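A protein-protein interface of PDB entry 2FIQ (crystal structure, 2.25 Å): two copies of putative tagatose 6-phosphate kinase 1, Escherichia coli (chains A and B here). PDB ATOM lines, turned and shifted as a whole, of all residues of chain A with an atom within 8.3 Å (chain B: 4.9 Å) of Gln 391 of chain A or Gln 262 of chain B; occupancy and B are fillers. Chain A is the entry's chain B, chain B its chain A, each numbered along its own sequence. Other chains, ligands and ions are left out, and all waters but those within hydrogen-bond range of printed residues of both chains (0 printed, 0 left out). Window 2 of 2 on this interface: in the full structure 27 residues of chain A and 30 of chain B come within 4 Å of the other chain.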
ATOM      1  N   LEU A 376      29.097   7.500  37.276  1.00  0.00           N
ATOM      2  CA  LEU A 376      28.236   7.094  36.189  1.00  0.00           C
ATOM      3  C   LEU A 376      26.905   6.527  36.691  1.00  0.00           C
ATOM      4  O   LEU A 376      25.829   6.880  36.186  1.00  0.00           O
ATOM      5  CB  LEU A 376      28.978   5.997  35.427  1.00  0.00           C
ATOM      6  CG  LEU A 376      29.111   6.235  33.938  1.00  0.00           C
ATOM      7  CD1 LEU A 376      29.931   7.523  33.684  1.00  0.00           C
ATOM      8  CD2 LEU A 376      29.732   4.967  33.286  1.00  0.00           C
ATOM      9  N   ILE A 379      24.145   8.939  37.620  1.00  0.00           N
ATOM     10  CA  ILE A 379      23.516   9.564  36.469  1.00  0.00           C
ATOM     11  C   ILE A 379      22.561   8.565  35.851  1.00  0.00           C
ATOM     12  O   ILE A 379      21.472   8.910  35.454  1.00  0.00           O
ATOM     13  CB  ILE A 379      24.591  10.052  35.471  1.00  0.00           C
ATOM     14  CG1 ILE A 379      25.409  11.182  36.137  1.00  0.00           C
ATOM     15  CG2 ILE A 379      23.971  10.501  34.138  1.00  0.00           C
ATOM     16  CD1 ILE A 379      26.578  11.649  35.311  1.00  0.00           C
ATOM     17  N   SER A 380      22.950   7.307  35.817  1.00  0.00           N
ATOM     18  CA  SER A 380      22.033   6.275  35.361  1.00  0.00           C
ATOM     19  C   SER A 380      20.804   6.243  36.287  1.00  0.00           C
ATOM     20  O   SER A 380      19.696   6.150  35.815  1.00  0.00           O
ATOM     21  CB  SER A 380      22.749   4.933  35.304  1.00  0.00           C
ATOM     22  OG  SER A 380      21.825   3.909  35.063  1.00  0.00           O
ATOM     23  N   PRO A 384      18.713   8.961  33.663  1.00  0.00           N
ATOM     24  CA  PRO A 384      19.050   7.849  32.752  1.00  0.00           C
ATOM     25  C   PRO A 384      19.224   8.169  31.260  1.00  0.00           C
ATOM     26  O   PRO A 384      20.105   7.590  30.621  1.00  0.00           O
ATOM     27  CB  PRO A 384      17.898   6.845  32.962  1.00  0.00           C
ATOM     28  CG  PRO A 384      16.849   7.561  33.659  1.00  0.00           C
ATOM     29  CD  PRO A 384      17.516   8.664  34.465  1.00  0.00           C
ATOM     30  N   LYS A 385      18.416   9.075  30.714  1.00  0.00           N
ATOM     31  CA  LYS A 385      18.547   9.481  29.307  1.00  0.00           C
ATOM     32  C   LYS A 385      19.870  10.230  29.032  1.00  0.00           C
ATOM     33  O   LYS A 385      20.454  10.106  27.947  1.00  0.00           O
ATOM     34  CB  LYS A 385      17.338  10.322  28.868  1.00  0.00           C
ATOM     35  CG  LYS A 385      16.029   9.520  28.824  1.00  0.00           C
ATOM     36  CD  LYS A 385      14.876  10.240  28.171  1.00  0.00           C
ATOM     37  CE  LYS A 385      15.069  10.498  26.667  1.00  0.00           C
ATOM     38  NZ  LYS A 385      15.773   9.322  26.087  1.00  0.00           N
ATOM     39  N   GLN A 386      20.348  10.981  30.027  1.00  0.00           N
ATOM     40  CA  GLN A 386      21.659  11.637  29.951  1.00  0.00           C
ATOM     41  C   GLN A 386      22.784  10.614  30.045  1.00  0.00           C
ATOM     42  O   GLN A 386      23.814  10.741  29.372  1.00  0.00           O
ATOM     43  CB  GLN A 386      21.802  12.697  31.050  1.00  0.00           C
ATOM     44  CG  GLN A 386      20.987  13.968  30.810  1.00  0.00           C
ATOM     45  CD  GLN A 386      19.472  13.752  30.820  1.00  0.00           C
ATOM     46  OE1 GLN A 386      18.915  13.229  31.780  1.00  0.00           O
ATOM     47  NE2 GLN A 386      18.795  14.166  29.738  1.00  0.00           N
ATOM     48  N   PHE A 387      22.585   9.600  30.884  1.00  0.00           N
ATOM     49  CA  PHE A 387      23.541   8.526  31.007  1.00  0.00           C
ATOM     50  C   PHE A 387      23.704   7.757  29.674  1.00  0.00           C
ATOM     51  O   PHE A 387      24.802   7.362  29.298  1.00  0.00           O
ATOM     52  CB  PHE A 387      23.124   7.567  32.123  1.00  0.00           C
ATOM     53  CG  PHE A 387      23.929   6.315  32.157  1.00  0.00           C
ATOM     54  CD1 PHE A 387      25.142   6.281  32.826  1.00  0.00           C
ATOM     55  CD2 PHE A 387      23.494   5.164  31.485  1.00  0.00           C
ATOM     56  CE1 PHE A 387      25.917   5.112  32.845  1.00  0.00           C
ATOM     57  CE2 PHE A 387      24.273   3.988  31.502  1.00  0.00           C
ATOM     58  CZ  PHE A 387      25.479   3.965  32.182  1.00  0.00           C
ATOM     59  N   GLU A 388      22.606   7.519  28.980  1.00  0.00           N
ATOM     60  CA  GLU A 388      22.685   6.832  27.701  1.00  0.00           C
ATOM     61  C   GLU A 388      23.526   7.644  26.717  1.00  0.00           C
ATOM     62  O   GLU A 388      24.353   7.077  26.004  1.00  0.00           O
ATOM     63  CB  GLU A 388      21.291   6.552  27.164  1.00  0.00           C
ATOM     64  CG  GLU A 388      20.567   5.461  27.947  1.00  0.00           C
ATOM     65  CD  GLU A 388      19.106   5.235  27.483  1.00  0.00           C
ATOM     66  OE1 GLU A 388      18.562   6.015  26.658  1.00  0.00           O
ATOM     67  OE2 GLU A 388      18.498   4.262  27.977  1.00  0.00           O
ATOM     68  N   ARG A 389      23.341   8.967  26.721  1.00  0.00           N
ATOM     69  CA  ARG A 389      24.126   9.863  25.878  1.00  0.00           C
ATOM     70  C   ARG A 389      25.618   9.849  26.205  1.00  0.00           C
ATOM     71  O   ARG A 389      26.449   9.738  25.308  1.00  0.00           O
ATOM     72  CB  ARG A 389      23.542  11.283  25.896  1.00  0.00           C
ATOM     73  CG  ARG A 389      22.137  11.255  25.369  1.00  0.00           C
ATOM     74  CD  ARG A 389      21.686  12.538  24.716  1.00  0.00           C
ATOM     75  NE  ARG A 389      20.441  12.251  24.008  1.00  0.00           N
ATOM     76  CZ  ARG A 389      19.220  12.330  24.550  1.00  0.00           C
ATOM     77  NH1 ARG A 389      19.070  12.751  25.827  1.00  0.00           N
ATOM     78  NH2 ARG A 389      18.140  12.009  23.797  1.00  0.00           N
ATOM     79  N   ILE A 390      25.950   9.919  27.486  1.00  0.00           N
ATOM     80  CA  ILE A 390      27.326   9.745  27.918  1.00  0.00           C
ATOM     81  C   ILE A 390      27.849   8.367  27.467  1.00  0.00           C
ATOM     82  O   ILE A 390      28.953   8.264  26.930  1.00  0.00           O
ATOM     83  CB  ILE A 390      27.476   9.951  29.460  1.00  0.00           C
ATOM     84  CG1 ILE A 390      27.046  11.374  29.862  1.00  0.00           C
ATOM     85  CG2 ILE A 390      28.897   9.657  29.914  1.00  0.00           C
ATOM     86  CD1 ILE A 390      26.638  11.513  31.319  1.00  0.00           C
ATOM     87  N   GLN A 391      27.037   7.327  27.662  1.00  0.00           N
ATOM     88  CA  GLN A 391      27.392   5.935  27.333  1.00  0.00           C
ATOM     89  C   GLN A 391      27.810   5.809  25.852  1.00  0.00           C
ATOM     90  O   GLN A 391      28.750   5.080  25.518  1.00  0.00           O
ATOM     91  CB  GLN A 391      26.203   5.013  27.640  1.00  0.00           C
ATOM     92  CG  GLN A 391      26.534   3.577  28.032  1.00  0.00           C
ATOM     93  CD  GLN A 391      25.315   2.619  27.922  1.00  0.00           C
ATOM     94  OE1 GLN A 391      24.327   2.906  27.224  1.00  0.00           O
ATOM     95  NE2 GLN A 391      25.389   1.484  28.624  1.00  0.00           N
ATOM     96  N   SER A 392      27.118   6.555  24.989  1.00  0.00           N
ATOM     97  CA  SER A 392      27.406   6.588  23.571  1.00  0.00           C
ATOM     98  C   SER A 392      28.339   7.760  23.192  1.00  0.00           C
ATOM     99  O   SER A 392      28.518   8.068  22.005  1.00  0.00           O
ATOM    100  CB  SER A 392      26.096   6.636  22.787  1.00  0.00           C
ATOM    101  OG  SER A 392      25.499   7.916  22.870  1.00  0.00           O
ATOM    102  N   GLY A 393      28.932   8.397  24.207  1.00  0.00           N
ATOM    103  CA  GLY A 393      29.936   9.448  24.013  1.00  0.00           C
ATOM    104  C   GLY A 393      29.483  10.712  23.298  1.00  0.00           C
ATOM    105  O   GLY A 393      30.286  11.365  22.635  1.00  0.00           O
ATOM    106  N   GLU A 394      28.206  11.069  23.427  1.00  0.00           N
ATOM    107  CA  GLU A 394      27.696  12.311  22.829  1.00  0.00           C
ATOM    108  C   GLU A 394      27.297  13.396  23.841  1.00  0.00           C
ATOM    109  O   GLU A 394      26.555  14.329  23.511  1.00  0.00           O
ATOM    110  CB  GLU A 394      26.561  12.017  21.831  1.00  0.00           C
ATOM    111  CG  GLU A 394      25.377  11.205  22.376  1.00  0.00           C
ATOM    112  CD  GLU A 394      24.581  10.467  21.276  1.00  0.00           C
ATOM    113  OE1 GLU A 394      24.952  10.586  20.085  1.00  0.00           O
ATOM    114  OE2 GLU A 394      23.595   9.753  21.613  1.00  0.00           O
ATOM    115  N   LEU A 395      27.808  13.270  25.062  1.00  0.00           N
ATOM    116  CA  LEU A 395      27.494  14.159  26.187  1.00  0.00           C
ATOM    117  C   LEU A 395      28.477  13.839  27.323  1.00  0.00           C
ATOM    118  O   LEU A 395      28.974  12.715  27.403  1.00  0.00           O
ATOM    119  CB  LEU A 395      26.039  13.936  26.656  1.00  0.00           C
ATOM    120  CG  LEU A 395      25.480  14.699  27.871  1.00  0.00           C
ATOM    121  CD1 LEU A 395      25.373  16.175  27.562  1.00  0.00           C
ATOM    122  CD2 LEU A 395      24.137  14.120  28.369  1.00  0.00           C
ATOM    123  N   SER A 396      28.761  14.818  28.183  1.00  0.00           N
ATOM    124  CA  SER A 396      29.605  14.575  29.360  1.00  0.00           C
ATOM    125  C   SER A 396      28.832  14.692  30.673  1.00  0.00           C
ATOM    126  O   SER A 396      27.685  15.150  30.699  1.00  0.00           O
ATOM    127  CB  SER A 396      30.831  15.505  29.375  1.00  0.00           C
ATOM    128  OG  SER A 396      31.973  14.885  28.808  1.00  0.00           O
ATOM    129  N   VAL B 225      35.942  -6.342  26.237  1.00  0.00           N
ATOM    130  CA  VAL B 225      34.836  -5.780  27.033  1.00  0.00           C
ATOM    131  C   VAL B 225      34.941  -6.094  28.527  1.00  0.00           C
ATOM    132  O   VAL B 225      35.261  -7.220  28.924  1.00  0.00           O
ATOM    133  CB  VAL B 225      33.425  -6.187  26.487  1.00  0.00           C
ATOM    134  CG1 VAL B 225      33.255  -5.726  25.056  1.00  0.00           C
ATOM    135  CG2 VAL B 225      33.206  -7.671  26.585  1.00  0.00           C
ATOM    136  N   GLU B 226      34.634  -5.092  29.342  1.00  0.00           N
ATOM    137  CA  GLU B 226      34.651  -5.207  30.791  1.00  0.00           C
ATOM    138  C   GLU B 226      34.024  -3.996  31.424  1.00  0.00           C
ATOM    139  O   GLU B 226      33.851  -2.958  30.781  1.00  0.00           O
ATOM    140  CB  GLU B 226      36.082  -5.282  31.320  1.00  0.00           C
ATOM    141  CG  GLU B 226      36.448  -6.615  31.941  1.00  0.00           C
ATOM    142  CD  GLU B 226      37.765  -6.561  32.719  1.00  0.00           C
ATOM    143  OE1 GLU B 226      38.162  -5.469  33.192  1.00  0.00           O
ATOM    144  OE2 GLU B 226      38.405  -7.627  32.856  1.00  0.00           O
ATOM    145  N   ILE B 232      33.311   1.475  32.143  1.00  0.00           N
ATOM    146  CA  ILE B 232      33.043   0.473  31.130  1.00  0.00           C
ATOM    147  C   ILE B 232      34.175   0.475  30.096  1.00  0.00           C
ATOM    148  O   ILE B 232      34.597   1.542  29.622  1.00  0.00           O
ATOM    149  CB  ILE B 232      31.684   0.734  30.431  1.00  0.00           C
ATOM    150  CG1 ILE B 232      30.568   0.930  31.471  1.00  0.00           C
ATOM    151  CG2 ILE B 232      31.351  -0.412  29.424  1.00  0.00           C
ATOM    152  CD1 ILE B 232      29.427   1.803  31.012  1.00  0.00           C
ATOM    153  N   ILE B 233      34.668  -0.721  29.765  1.00  0.00           N
ATOM    154  CA  ILE B 233      35.604  -0.908  28.643  1.00  0.00           C
ATOM    155  C   ILE B 233      34.775  -1.252  27.421  1.00  0.00           C
ATOM    156  O   ILE B 233      34.232  -2.344  27.309  1.00  0.00           O
ATOM    157  CB  ILE B 233      36.654  -2.022  28.908  1.00  0.00           C
ATOM    158  CG1 ILE B 233      37.389  -1.765  30.239  1.00  0.00           C
ATOM    159  CG2 ILE B 233      37.633  -2.168  27.717  1.00  0.00           C
ATOM    160  CD1 ILE B 233      38.124  -0.421  30.342  1.00  0.00           C
ATOM    161  N   HIS B 234      34.664  -0.282  26.526  1.00  0.00           N
ATOM    162  CA  HIS B 234      33.821  -0.398  25.365  1.00  0.00           C
ATOM    163  C   HIS B 234      34.514  -1.189  24.277  1.00  0.00           C
ATOM    164  O   HIS B 234      35.717  -1.018  24.012  1.00  0.00           O
ATOM    165  CB  HIS B 234      33.409   0.991  24.874  1.00  0.00           C
ATOM    166  CG  HIS B 234      32.576   1.749  25.863  1.00  0.00           C
ATOM    167  ND1 HIS B 234      31.233   1.499  26.054  1.00  0.00           N
ATOM    168  CD2 HIS B 234      32.903   2.737  26.734  1.00  0.00           C
ATOM    169  CE1 HIS B 234      30.762   2.311  26.983  1.00  0.00           C
ATOM    170  NE2 HIS B 234      31.755   3.070  27.415  1.00  0.00           N
ATOM    171  N   TYR B 235      33.744  -2.076  23.664  1.00  0.00           N
ATOM    172  CA  TYR B 235      34.218  -2.887  22.557  1.00  0.00           C
ATOM    173  C   TYR B 235      34.881  -2.058  21.473  1.00  0.00           C
ATOM    174  O   TYR B 235      34.317  -1.068  21.018  1.00  0.00           O
ATOM    175  CB  TYR B 235      33.040  -3.652  21.940  1.00  0.00           C
ATOM    176  CG  TYR B 235      33.432  -4.568  20.806  1.00  0.00           C
ATOM    177  CD1 TYR B 235      34.496  -5.448  20.947  1.00  0.00           C
ATOM    178  CD2 TYR B 235      32.702  -4.587  19.597  1.00  0.00           C
ATOM    179  CE1 TYR B 235      34.853  -6.318  19.911  1.00  0.00           C
ATOM    180  CE2 TYR B 235      33.057  -5.470  18.542  1.00  0.00           C
ATOM    181  CZ  TYR B 235      34.143  -6.311  18.719  1.00  0.00           C
ATOM    182  OH  TYR B 235      34.526  -7.191  17.733  1.00  0.00           O
ATOM    183  N   THR B 259      29.564  -8.819  29.285  1.00  0.00           N
ATOM    184  CA  THR B 259      29.232  -7.945  28.159  1.00  0.00           C
ATOM    185  C   THR B 259      28.299  -6.790  28.587  1.00  0.00           C
ATOM    186  O   THR B 259      27.875  -5.970  27.776  1.00  0.00           O
ATOM    187  CB  THR B 259      28.637  -8.742  26.980  1.00  0.00           C
ATOM    188  OG1 THR B 259      27.323  -9.189  27.312  1.00  0.00           O
ATOM    189  CG2 THR B 259      29.514  -9.960  26.652  1.00  0.00           C
ATOM    190  N   ASP B 260      28.013  -6.754  29.884  1.00  0.00           N
ATOM    191  CA  ASP B 260      27.124  -5.778  30.497  1.00  0.00           C
ATOM    192  C   ASP B 260      27.553  -4.329  30.234  1.00  0.00           C
ATOM    193  O   ASP B 260      28.736  -4.003  30.259  1.00  0.00           O
ATOM    194  CB  ASP B 260      27.049  -6.028  32.010  1.00  0.00           C
ATOM    195  CG  ASP B 260      26.812  -7.494  32.362  1.00  0.00           C
ATOM    196  OD1 ASP B 260      27.643  -8.373  32.035  1.00  0.00           O
ATOM    197  OD2 ASP B 260      25.776  -7.766  32.977  1.00  0.00           O
ATOM    198  N   TYR B 261      26.563  -3.476  29.980  1.00  0.00           N
ATOM    199  CA  TYR B 261      26.732  -2.027  29.902  1.00  0.00           C
ATOM    200  C   TYR B 261      27.339  -1.509  28.576  1.00  0.00           C
ATOM    201  O   TYR B 261      27.754  -0.355  28.482  1.00  0.00           O
ATOM    202  CB  TYR B 261      27.526  -1.515  31.116  1.00  0.00           C
ATOM    203  CG  TYR B 261      27.040  -2.003  32.476  1.00  0.00           C
ATOM    204  CD1 TYR B 261      25.803  -1.588  33.003  1.00  0.00           C
ATOM    205  CD2 TYR B 261      27.835  -2.859  33.253  1.00  0.00           C
ATOM    206  CE1 TYR B 261      25.378  -2.025  34.245  1.00  0.00           C
ATOM    207  CE2 TYR B 261      27.422  -3.288  34.509  1.00  0.00           C
ATOM    208  CZ  TYR B 261      26.190  -2.867  34.996  1.00  0.00           C
ATOM    209  OH  TYR B 261      25.783  -3.297  36.239  1.00  0.00           O
ATOM    210  N   GLN B 262      27.404  -2.348  27.548  1.00  0.00           N
ATOM    211  CA  GLN B 262      27.881  -1.870  26.259  1.00  0.00           C
ATOM    212  C   GLN B 262      26.770  -1.106  25.534  1.00  0.00           C
ATOM    213  O   GLN B 262      25.596  -1.241  25.855  1.00  0.00           O
ATOM    214  CB  GLN B 262      28.390  -3.028  25.409  1.00  0.00           C
ATOM    215  CG  GLN B 262      29.521  -3.843  26.050  1.00  0.00           C
ATOM    216  CD  GLN B 262      30.849  -3.123  26.022  1.00  0.00           C
ATOM    217  OE1 GLN B 262      31.164  -2.430  25.052  1.00  0.00           O
ATOM    218  NE2 GLN B 262      31.626  -3.254  27.101  1.00  0.00           N
ATOM    219  N   THR B 263      27.125  -0.279  24.567  1.00  0.00           N
ATOM    220  CA  THR B 263      26.104   0.352  23.729  1.00  0.00           C
ATOM    221  C   THR B 263      25.441  -0.710  22.817  1.00  0.00           C
ATOM    222  O   THR B 263      26.023  -1.780  22.526  1.00  0.00           O
ATOM    223  CB  THR B 263      26.702   1.451  22.832  1.00  0.00           C
ATOM    224  OG1 THR B 263      27.552   0.827  21.868  1.00  0.00           O
ATOM    225  CG2 THR B 263      27.506   2.496  23.665  1.00  0.00           C
ATOM    226  N   ARG B 264      24.223  -0.419  22.370  1.00  0.00           N
ATOM    227  CA  ARG B 264      23.542  -1.329  21.480  1.00  0.00           C
ATOM    228  C   ARG B 264      24.265  -1.463  20.137  1.00  0.00           C
ATOM    229  O   ARG B 264      24.166  -2.484  19.486  1.00  0.00           O
ATOM    230  CB  ARG B 264      22.052  -0.981  21.361  1.00  0.00           C
ATOM    231  CG  ARG B 264      21.696   0.249  20.558  1.00  0.00           C
ATOM    232  CD  ARG B 264      20.183   0.320  20.386  1.00  0.00           C
ATOM    233  NE  ARG B 264      19.507   0.260  21.683  1.00  0.00           N
ATOM    234  CZ  ARG B 264      18.236  -0.100  21.885  1.00  0.00           C
ATOM    235  NH1 ARG B 264      17.444  -0.462  20.874  1.00  0.00           N
ATOM    236  NH2 ARG B 264      17.760  -0.102  23.127  1.00  0.00           N
ATOM    237  N   ALA B 266      27.616  -1.596  19.947  1.00  0.00           N
ATOM    238  CA  ALA B 266      28.648  -2.585  20.302  1.00  0.00           C
ATOM    239  C   ALA B 266      28.113  -3.997  20.276  1.00  0.00           C
ATOM    240  O   ALA B 266      28.797  -4.872  19.810  1.00  0.00           O
ATOM    241  CB  ALA B 266      29.265  -2.272  21.674  1.00  0.00           C
ATOM    242  N   TYR B 267      26.894  -4.226  20.770  1.00  0.00           N
ATOM    243  CA  TYR B 267      26.294  -5.566  20.722  1.00  0.00           C
ATOM    244  C   TYR B 267      26.102  -6.061  19.295  1.00  0.00           C
ATOM    245  O   TYR B 267      26.277  -7.245  19.004  1.00  0.00           O
ATOM    246  CB  TYR B 267      24.945  -5.624  21.448  1.00  0.00           C
ATOM    247  CG  TYR B 267      25.062  -5.415  22.918  1.00  0.00           C
ATOM    248  CD1 TYR B 267      26.020  -6.109  23.664  1.00  0.00           C
ATOM    249  CD2 TYR B 267      24.227  -4.517  23.576  1.00  0.00           C
ATOM    250  CE1 TYR B 267      26.156  -5.890  25.035  1.00  0.00           C
ATOM    251  CE2 TYR B 267      24.363  -4.290  24.948  1.00  0.00           C
ATOM    252  CZ  TYR B 267      25.324  -4.989  25.665  1.00  0.00           C
ATOM    253  OH  TYR B 267      25.439  -4.780  27.016  1.00  0.00           O
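O of Tyr 261 of chain B sits at hydrogen-bond distance from NE2 of Gln 391 of chain A (3.0 Å).
Of chain B, only His 234, Tyr 261, Gln 262 and Thr 263 come within 4 Å of Gln 391 of chain A. Of the printed residues of chain A, Gln 262 of chain B touches Gln 391 (3.9 Å). Thr 263 of chain B touches one residue of chain A. Of the printed residues of chain B, Leu 376 of chain A touches Ile 232. Of the printed residues of chain A, His 234 of chain B touches Gln 391 (3.7 Å). Gly 393 of chain A touches none of the printed residues of chain B. Gln 386 of chain A touches none of the printed residues of chain B. The nearest residue of chain B that does not touch Gln 391 of chain A is Ile 232 of chain B (4.5 Å). The nearest residue of chain A that does not touch Gln 262 of chain B is Ser 392 of chain A (7.7 Å).
Among the printed residues, pairs that only touch across the chains: Leu 376 of chain A with Ile 232 of chain B, Gln 391 of chain A with His 234 of chain B, Gln 391 of chain A with Gln 262 of chain B and Gln 391 of chain A with Thr 263 of chain B.
No position is printed for both chains.
O of Ile 233 of chain B is in hydrogen-bond range of NE2 of Gln 262 of chain B, 2.8 Å away. The backbone NH (N) of Tyr 235 of chain B is in hydrogen-bond range of the side-chain amide oxygen (OE1) of Gln 262 of chain B, at 3.0 Å. N of Tyr 261 of chain B sits at hydrogen-bond distance from OH of Tyr 267 of chain B, at 3.4 Å. N of Gln 262 of chain B sits at hydrogen-bond distance from OH of Tyr 267 of chain B, at 3.2 Å. The backbone NH of Ala 266 of chain B sits at hydrogen-bond distance from the side-chain hydroxyl of Thr 263 of chain B, at 3.1 Å.
Printed residues of chain A that touch a printed residue of chain B: Leu 376 and Gln 391. Hydrophobic or aromatic side chains of chain A within 4 Å of the printed part of chain B: Leu 376. Along chain A the printed residues that touch a printed residue of chain B span positions 376 to 391. Of the 14 printed residues of chain B, 5 touch a printed residue of chain A. Hydrophobic or aromatic side chains of chain B that line the printed part of chain A: Ile 232 and His 234. Among the printed residues, 5 pairs touch across the chains. Among the printed residues, no Asp or Glu carboxylate lies within 4 Å of a Lys or Arg side-chain nitrogen of the other chain.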
